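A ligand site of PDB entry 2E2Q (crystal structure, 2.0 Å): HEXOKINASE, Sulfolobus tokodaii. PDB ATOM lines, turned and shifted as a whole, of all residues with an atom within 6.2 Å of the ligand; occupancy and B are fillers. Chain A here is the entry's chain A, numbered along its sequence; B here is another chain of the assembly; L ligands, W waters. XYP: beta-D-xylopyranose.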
ATOM      1  N   ASN A  35       7.099  13.503   4.762  1.00  0.00           N
ATOM      2  CA  ASN A  35       7.871  14.734   4.984  1.00  0.00           C
ATOM      3  C   ASN A  35       7.515  15.701   3.852  1.00  0.00           C
ATOM      4  O   ASN A  35       8.021  15.554   2.734  1.00  0.00           O
ATOM      5  CB  ASN A  35       9.374  14.408   4.953  1.00  0.00           C
ATOM      6  CG  ASN A  35      10.246  15.603   5.310  1.00  0.00           C
ATOM      7  OD1 ASN A  35       9.872  16.763   5.089  1.00  0.00           O
ATOM      8  ND2 ASN A  35      11.436  15.329   5.858  1.00  0.00           N
ATOM      9  N   HIS A  37       8.523  18.419   3.057  1.00  0.00           N
ATOM     10  CA  HIS A  37       9.654  19.137   2.472  1.00  0.00           C
ATOM     11  C   HIS A  37      10.189  18.347   1.290  1.00  0.00           C
ATOM     12  O   HIS A  37      10.814  18.901   0.393  1.00  0.00           O
ATOM     13  CB  HIS A  37      10.749  19.316   3.522  1.00  0.00           C
ATOM     14  CG  HIS A  37      10.404  20.304   4.583  1.00  0.00           C
ATOM     15  ND1 HIS A  37      10.723  20.116   5.912  1.00  0.00           N
ATOM     16  CD2 HIS A  37       9.766  21.507   4.520  1.00  0.00           C
ATOM     17  CE1 HIS A  37      10.292  21.149   6.619  1.00  0.00           C
ATOM     18  NE2 HIS A  37       9.710  22.008   5.792  1.00  0.00           N
ATOM     19  N   ASN A  38       9.916  17.041   1.300  1.00  0.00           N
ATOM     20  CA  ASN A  38      10.372  16.141   0.237  1.00  0.00           C
ATOM     21  C   ASN A  38       9.377  15.918  -0.900  1.00  0.00           C
ATOM     22  O   ASN A  38       9.782  15.752  -2.039  1.00  0.00           O
ATOM     23  CB  ASN A  38      10.725  14.774   0.833  1.00  0.00           C
ATOM     24  CG  ASN A  38      11.946  14.823   1.735  1.00  0.00           C
ATOM     25  OD1 ASN A  38      12.429  15.887   2.099  1.00  0.00           O
ATOM     26  ND2 ASN A  38      12.444  13.642   2.098  1.00  0.00           N
ATOM     27  N   VAL A  67       6.076  12.927  12.820  1.00  0.00           N
ATOM     28  CA  VAL A  67       6.316  13.407  11.475  1.00  0.00           C
ATOM     29  C   VAL A  67       7.710  13.987  11.227  1.00  0.00           C
ATOM     30  O   VAL A  67       8.180  14.853  11.976  1.00  0.00           O
ATOM     31  CB  VAL A  67       5.252  14.484  11.067  1.00  0.00           C
ATOM     32  CG1 VAL A  67       5.366  14.814   9.584  1.00  0.00           C
ATOM     33  CG2 VAL A  67       3.838  13.971  11.398  1.00  0.00           C
ATOM     34  N   ALA A  68       8.351  13.485  10.179  1.00  0.00           N
ATOM     35  CA  ALA A  68       9.663  13.971   9.783  1.00  0.00           C
ATOM     36  C   ALA A  68       9.411  15.286   9.057  1.00  0.00           C
ATOM     37  O   ALA A  68       8.446  15.404   8.304  1.00  0.00           O
ATOM     38  CB  ALA A  68      10.313  12.972   8.831  1.00  0.00           C
ATOM     39  N   GLY A  69      10.253  16.286   9.295  1.00  0.00           N
ATOM     40  CA  GLY A  69      10.068  17.562   8.618  1.00  0.00           C
ATOM     41  C   GLY A  69       9.482  18.680   9.462  1.00  0.00           C
ATOM     42  O   GLY A  69       9.485  19.818   9.025  1.00  0.00           O
ATOM     43  N   LEU A  70       8.957  18.379  10.644  1.00  0.00           N
ATOM     44  CA  LEU A  70       8.415  19.428  11.502  1.00  0.00           C
ATOM     45  C   LEU A  70       9.633  20.018  12.200  1.00  0.00           C
ATOM     46  O   LEU A  70       9.963  19.636  13.324  1.00  0.00           O
ATOM     47  CB  LEU A  70       7.431  18.851  12.522  1.00  0.00           C
ATOM     48  CG  LEU A  70       6.261  18.070  11.895  1.00  0.00           C
ATOM     49  CD1 LEU A  70       5.240  17.723  12.963  1.00  0.00           C
ATOM     50  CD2 LEU A  70       5.618  18.917  10.806  1.00  0.00           C
ATOM     51  N   ASP A  71      10.287  20.933  11.501  1.00  0.00           N
ATOM     52  CA  ASP A  71      11.533  21.538  11.984  1.00  0.00           C
ATOM     53  C   ASP A  71      11.479  23.049  12.228  1.00  0.00           C
ATOM     54  O   ASP A  71      12.525  23.699  12.287  1.00  0.00           O
ATOM     55  CB  ASP A  71      12.627  21.249  10.978  1.00  0.00           C
ATOM     56  CG  ASP A  71      12.649  19.802  10.540  1.00  0.00           C
ATOM     57  OD1 ASP A  71      13.068  19.522   9.403  1.00  0.00           O
ATOM     58  OD2 ASP A  71      12.242  18.943  11.353  1.00  0.00           O
ATOM     59  N   HIS A  94       6.948  15.334  16.583  1.00  0.00           N
ATOM     60  CA  HIS A  94       8.071  15.201  15.663  1.00  0.00           C
ATOM     61  C   HIS A  94       8.349  13.707  15.631  1.00  0.00           C
ATOM     62  O   HIS A  94       8.056  13.007  16.607  1.00  0.00           O
ATOM     63  CB  HIS A  94       9.279  15.961  16.198  1.00  0.00           C
ATOM     64  CG  HIS A  94      10.481  15.880  15.310  1.00  0.00           C
ATOM     65  ND1 HIS A  94      11.699  15.399  15.737  1.00  0.00           N
ATOM     66  CD2 HIS A  94      10.644  16.212  14.005  1.00  0.00           C
ATOM     67  CE1 HIS A  94      12.558  15.441  14.737  1.00  0.00           C
ATOM     68  NE2 HIS A  94      11.944  15.933  13.677  1.00  0.00           N
ATOM     69  N   ASP A  95       8.917  13.205  14.546  1.00  0.00           N
ATOM     70  CA  ASP A  95       9.175  11.774  14.457  1.00  0.00           C
ATOM     71  C   ASP A  95      10.195  11.269  15.478  1.00  0.00           C
ATOM     72  O   ASP A  95      10.165  10.097  15.843  1.00  0.00           O
ATOM     73  CB  ASP A  95       9.564  11.375  13.020  1.00  0.00           C
ATOM     74  CG  ASP A  95      10.926  11.919  12.568  1.00  0.00           C
ATOM     75  OD1 ASP A  95      11.352  12.990  13.030  1.00  0.00           O
ATOM     76  OD2 ASP A  95      11.552  11.254  11.728  1.00  0.00           O
ATOM     77  N   GLY A  96      11.052  12.155  15.955  1.00  0.00           N
ATOM     78  CA  GLY A  96      12.031  11.725  16.939  1.00  0.00           C
ATOM     79  C   GLY A  96      11.350  11.366  18.253  1.00  0.00           C
ATOM     80  O   GLY A  96      11.796  10.464  18.969  1.00  0.00           O
ATOM     81  N   ILE A 113      18.031   8.973  15.085  1.00  0.00           N
ATOM     82  CA  ILE A 113      17.308   8.507  13.905  1.00  0.00           C
ATOM     83  C   ILE A 113      18.227   8.698  12.714  1.00  0.00           C
ATOM     84  O   ILE A 113      18.778   9.784  12.501  1.00  0.00           O
ATOM     85  CB  ILE A 113      16.014   9.301  13.606  1.00  0.00           C
ATOM     86  CG1 ILE A 113      14.957   9.013  14.681  1.00  0.00           C
ATOM     87  CG2 ILE A 113      15.474   8.924  12.224  1.00  0.00           C
ATOM     88  CD1 ILE A 113      13.646   9.752  14.465  1.00  0.00           C
ATOM     89  N   THR A 116      16.026   8.559   6.016  1.00  0.00           N
ATOM     90  CA  THR A 116      16.221   9.413   4.838  1.00  0.00           C
ATOM     91  C   THR A 116      17.044  10.613   5.298  1.00  0.00           C
ATOM     92  O   THR A 116      17.953  11.071   4.604  1.00  0.00           O
ATOM     93  CB  THR A 116      14.875   9.895   4.264  1.00  0.00           C
ATOM     94  OG1 THR A 116      14.052   8.774   3.940  1.00  0.00           O
ATOM     95  CG2 THR A 116      15.104  10.720   2.996  1.00  0.00           C
ATOM     96  N   GLY A 117      16.702  11.112   6.486  1.00  0.00           N
ATOM     97  CA  GLY A 117      17.429  12.209   7.077  1.00  0.00           C
ATOM     98  C   GLY A 117      17.884  11.713   8.437  1.00  0.00           C
ATOM     99  O   GLY A 117      17.810  10.518   8.706  1.00  0.00           O
ATOM    100  N   SER A 118      18.345  12.606   9.314  1.00  0.00           N
ATOM    101  CA  SER A 118      18.789  12.170  10.621  1.00  0.00           C
ATOM    102  C   SER A 118      18.550  13.216  11.691  1.00  0.00           C
ATOM    103  O   SER A 118      18.379  14.405  11.407  1.00  0.00           O
ATOM    104  CB  SER A 118      20.274  11.810  10.606  1.00  0.00           C
ATOM    105  OG  SER A 118      21.066  12.964  10.383  1.00  0.00           O
ATOM    106  N   VAL A 119      18.550  12.766  12.933  1.00  0.00           N
ATOM    107  CA  VAL A 119      18.351  13.675  14.051  1.00  0.00           C
ATOM    108  C   VAL A 119      18.729  12.968  15.344  1.00  0.00           C
ATOM    109  O   VAL A 119      18.742  11.748  15.418  1.00  0.00           O
ATOM    110  CB  VAL A 119      16.861  14.133  14.121  1.00  0.00           C
ATOM    111  CG1 VAL A 119      15.960  12.958  14.475  1.00  0.00           C
ATOM    112  CG2 VAL A 119      16.699  15.264  15.163  1.00  0.00           C
ATOM    113  N   GLU A 121      17.497  13.297  19.169  1.00  0.00           N
ATOM    114  CA  GLU A 121      16.507  13.971  20.000  1.00  0.00           C
ATOM    115  C   GLU A 121      16.419  13.329  21.377  1.00  0.00           C
ATOM    116  O   GLU A 121      16.534  12.111  21.502  1.00  0.00           O
ATOM    117  CB  GLU A 121      15.144  13.960  19.308  1.00  0.00           C
ATOM    118  CG  GLU A 121      14.043  14.705  20.056  1.00  0.00           C
ATOM    119  CD  GLU A 121      12.919  15.181  19.135  1.00  0.00           C
ATOM    120  OE1 GLU A 121      12.700  14.553  18.080  1.00  0.00           O
ATOM    121  OE2 GLU A 121      12.264  16.190  19.467  1.00  0.00           O
ATOM    122  N   ARG A 130      16.963  18.692  20.633  1.00  0.00           N
ATOM    123  CA  ARG A 130      17.405  18.020  19.419  1.00  0.00           C
ATOM    124  C   ARG A 130      18.619  18.727  18.832  1.00  0.00           C
ATOM    125  O   ARG A 130      18.850  19.910  19.071  1.00  0.00           O
ATOM    126  CB  ARG A 130      16.286  17.969  18.367  1.00  0.00           C
ATOM    127  CG  ARG A 130      16.408  19.028  17.264  1.00  0.00           C
ATOM    128  CD  ARG A 130      15.612  18.684  16.002  1.00  0.00           C
ATOM    129  NE  ARG A 130      14.163  18.791  16.201  1.00  0.00           N
ATOM    130  CZ  ARG A 130      13.277  18.870  15.219  1.00  0.00           C
ATOM    131  NH1 ARG A 130      13.661  18.863  13.950  1.00  0.00           N
ATOM    132  NH2 ARG A 130      11.980  18.965  15.498  1.00  0.00           N
ATOM    133  N   GLY A 133      18.756  17.326  12.379  1.00  0.00           N
ATOM    134  CA  GLY A 133      17.351  17.145  12.035  1.00  0.00           C
ATOM    135  C   GLY A 133      16.698  18.392  11.464  1.00  0.00           C
ATOM    136  O   GLY A 133      15.563  18.721  11.820  1.00  0.00           O
ATOM    137  N   ARG A 134      17.414  19.075  10.576  1.00  0.00           N
ATOM    138  CA  ARG A 134      16.893  20.295   9.952  1.00  0.00           C
ATOM    139  C   ARG A 134      16.963  20.243   8.425  1.00  0.00           C
ATOM    140  O   ARG A 134      17.239  21.259   7.781  1.00  0.00           O
ATOM    141  CB  ARG A 134      17.674  21.518  10.452  1.00  0.00           C
ATOM    142  CG  ARG A 134      17.769  21.667  11.967  1.00  0.00           C
ATOM    143  CD  ARG A 134      16.426  21.998  12.608  1.00  0.00           C
ATOM    144  NE  ARG A 134      16.546  22.094  14.060  1.00  0.00           N
ATOM    145  CZ  ARG A 134      15.545  22.380  14.890  1.00  0.00           C
ATOM    146  NH1 ARG A 134      15.776  22.440  16.200  1.00  0.00           N
ATOM    147  NH2 ARG A 134      14.332  22.624  14.424  1.00  0.00           N
ATOM    148  N   GLY A 135      16.731  19.074   7.837  1.00  0.00           N
ATOM    149  CA  GLY A 135      16.772  18.981   6.381  1.00  0.00           C
ATOM    150  C   GLY A 135      18.074  18.507   5.762  1.00  0.00           C
ATOM    151  O   GLY A 135      19.135  18.558   6.394  1.00  0.00           O
ATOM    152  N   TRP A 136      17.998  18.093   4.510  1.00  0.00           N
ATOM    153  CA  TRP A 136      19.141  17.545   3.802  1.00  0.00           C
ATOM    154  C   TRP A 136      20.250  18.517   3.429  1.00  0.00           C
ATOM    155  O   TRP A 136      21.413  18.122   3.372  1.00  0.00           O
ATOM    156  CB  TRP A 136      18.688  16.786   2.537  1.00  0.00           C
ATOM    157  CG  TRP A 136      17.895  17.610   1.546  1.00  0.00           C
ATOM    158  CD1 TRP A 136      16.529  17.750   1.503  1.00  0.00           C
ATOM    159  CD2 TRP A 136      18.415  18.424   0.487  1.00  0.00           C
ATOM    160  NE1 TRP A 136      16.181  18.592   0.481  1.00  0.00           N
ATOM    161  CE2 TRP A 136      17.316  19.026  -0.161  1.00  0.00           C
ATOM    162  CE3 TRP A 136      19.711  18.698   0.022  1.00  0.00           C
ATOM    163  CZ2 TRP A 136      17.473  19.888  -1.255  1.00  0.00           C
ATOM    164  CZ3 TRP A 136      19.868  19.560  -1.072  1.00  0.00           C
ATOM    165  CH2 TRP A 136      18.751  20.140  -1.698  1.00  0.00           C
ATOM    166  N   SER A 139      21.539  19.867   7.290  1.00  0.00           N
ATOM    167  CA  SER A 139      22.005  18.818   8.201  1.00  0.00           C
ATOM    168  C   SER A 139      21.952  17.392   7.658  1.00  0.00           C
ATOM    169  O   SER A 139      22.466  17.109   6.582  1.00  0.00           O
ATOM    170  CB  SER A 139      21.214  18.894   9.521  1.00  0.00           C
ATOM    171  OG  SER A 139      19.825  18.716   9.291  1.00  0.00           O
ATOM    172  N   ASP A 140      21.333  16.510   8.433  1.00  0.00           N
ATOM    173  CA  ASP A 140      21.206  15.092   8.074  1.00  0.00           C
ATOM    174  C   ASP A 140      22.533  14.341   7.901  1.00  0.00           C
ATOM    175  O   ASP A 140      22.675  13.486   7.018  1.00  0.00           O
ATOM    176  CB  ASP A 140      20.314  14.931   6.836  1.00  0.00           C
ATOM    177  CG  ASP A 140      18.851  15.278   7.127  1.00  0.00           C
ATOM    178  OD1 ASP A 140      18.520  15.435   8.318  1.00  0.00           O
ATOM    179  OD2 ASP A 140      18.034  15.371   6.197  1.00  0.00           O
ATOM    180  N   TYR B 189      14.738  25.520   3.192  1.00  0.00           N
ATOM    181  CA  TYR B 189      13.667  24.792   2.524  1.00  0.00           C
ATOM    182  C   TYR B 189      13.021  25.550   1.361  1.00  0.00           C
ATOM    183  O   TYR B 189      12.267  24.983   0.580  1.00  0.00           O
ATOM    184  CB  TYR B 189      12.600  24.388   3.544  1.00  0.00           C
ATOM    185  CG  TYR B 189      13.008  23.209   4.392  1.00  0.00           C
ATOM    186  CD1 TYR B 189      13.424  22.008   3.811  1.00  0.00           C
ATOM    187  CD2 TYR B 189      12.977  23.287   5.787  1.00  0.00           C
ATOM    188  CE1 TYR B 189      13.807  20.924   4.587  1.00  0.00           C
ATOM    189  CE2 TYR B 189      13.351  22.209   6.580  1.00  0.00           C
ATOM    190  CZ  TYR B 189      13.762  21.029   5.977  1.00  0.00           C
ATOM    191  OH  TYR B 189      14.088  19.935   6.763  1.00  0.00           O
HETATM  192  O1  XYP L   1      15.493  15.568   7.324  1.00  0.00           O
HETATM  193  C1  XYP L   1      15.328  15.344   8.683  1.00  0.00           C
HETATM  194  C2  XYP L   1      14.129  16.148   9.183  1.00  0.00           C
HETATM  195  C3  XYP L   1      13.865  15.800  10.668  1.00  0.00           C
HETATM  196  C4  XYP L   1      13.707  14.293  10.834  1.00  0.00           C
HETATM  197  C5  XYP L   1      14.921  13.577  10.250  1.00  0.00           C
HETATM  198  O2  XYP L   1      14.401  17.530   9.050  1.00  0.00           O
HETATM  199  O3  XYP L   1      12.695  16.464  11.117  1.00  0.00           O
HETATM  200  O4  XYP L   1      13.589  13.967  12.207  1.00  0.00           O
HETATM  201  O5  XYP L   1      15.094  13.945   8.865  1.00  0.00           O
HETATM  202  O   HOH W   1      13.337  17.681   6.038  1.00  0.00           O
HETATM  203  O   HOH W   2      13.256  13.146   6.517  1.00  0.00           O
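OD1 of Asp 71 sits at hydrogen-bond distance from O2 of the ligand (2.4 Å). OD1 of Asp 95 sits at hydrogen-bond distance from O4 of the ligand (2.6 Å). A ring nitrogen (NE2) of His 94 is in hydrogen-bond range of an oxygen (O3) of the ligand, 2.7 Å away. O1 of the ligand sits at hydrogen-bond distance from OD2 of Asp 140, at 2.8 Å. The backbone NH (N) of Gly 135 sits at hydrogen-bond distance from an oxygen (O2) of the ligand (3.0 Å). The backbone NH (N) of Gly 69 is in hydrogen-bond range of an oxygen (O3) of the ligand. The backbone carbonyl oxygen of Gly 133 lies within hydrogen-bond range of an oxygen (O2) of the ligand (3.2 Å). OH of Tyr 189 of chain B sits at hydrogen-bond distance from O2 of the ligand, 3.3 Å away.
The backbone carbonyl oxygen (O) of Val 67 is in hydrogen-bond range of the backbone NH (N) of Asp 95 (3.1 Å). ND1 of His 94 lies close to N of Gly 96 (3.3 Å). N of Ser 118 lies within hydrogen-bond range of OD1 of Asp 140, at 3.0 Å. The side-chain hydroxyl (OH) of Tyr 189 of chain B lies close to the backbone NH (N) of Gly 135, 3.0 Å away. OG of Ser 139 is in hydrogen-bond range of O of Gly 135 (3.0 Å). O of Gly 69 sits close to ND1 of His 37 (3.4 Å). O of Gly 133 is in hydrogen-bond range of NH1 of Arg 130, 2.9 Å away. The side-chain hydroxyl (OH) of Tyr 189 of chain B lies close to a ring nitrogen (ND1) of His 37 (3.5 Å).
Merely in contact with the ligand: Gly 117 (3.4 Å), Val 119 (3.4 Å), Ser 118 (3.5 Å), Arg 134 (3.7 Å) and Arg 130 (3.8 Å). Hydrophobic or aromatic side chains that line the ligand: His 94 and Val 119. Within 4 Å of the ligand: Gly 69, Asp 71, His 94, Asp 95, Gly 117, Ser 118, Val 119, Arg 130, Gly 133, Arg 134, Gly 135, Asp 140 and Tyr 189 of chain B. The nearest printed residue that does not touch the ligand is Ala 68 (4.1 Å).
Water W2 bridges the side-chain amide nitrogen of Asn 35 (2.9 Å) and an oxygen (O5) of the ligand (3.1 Å). Water W1 lies within hydrogen-bond range of the side-chain hydroxyl (OH) of Tyr 189 of chain B (2.5 Å), the side-chain amide nitrogen (ND2) of Asn 35 (3.0 Å) and an oxygen (O2) of the ligand (3.2 Å).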
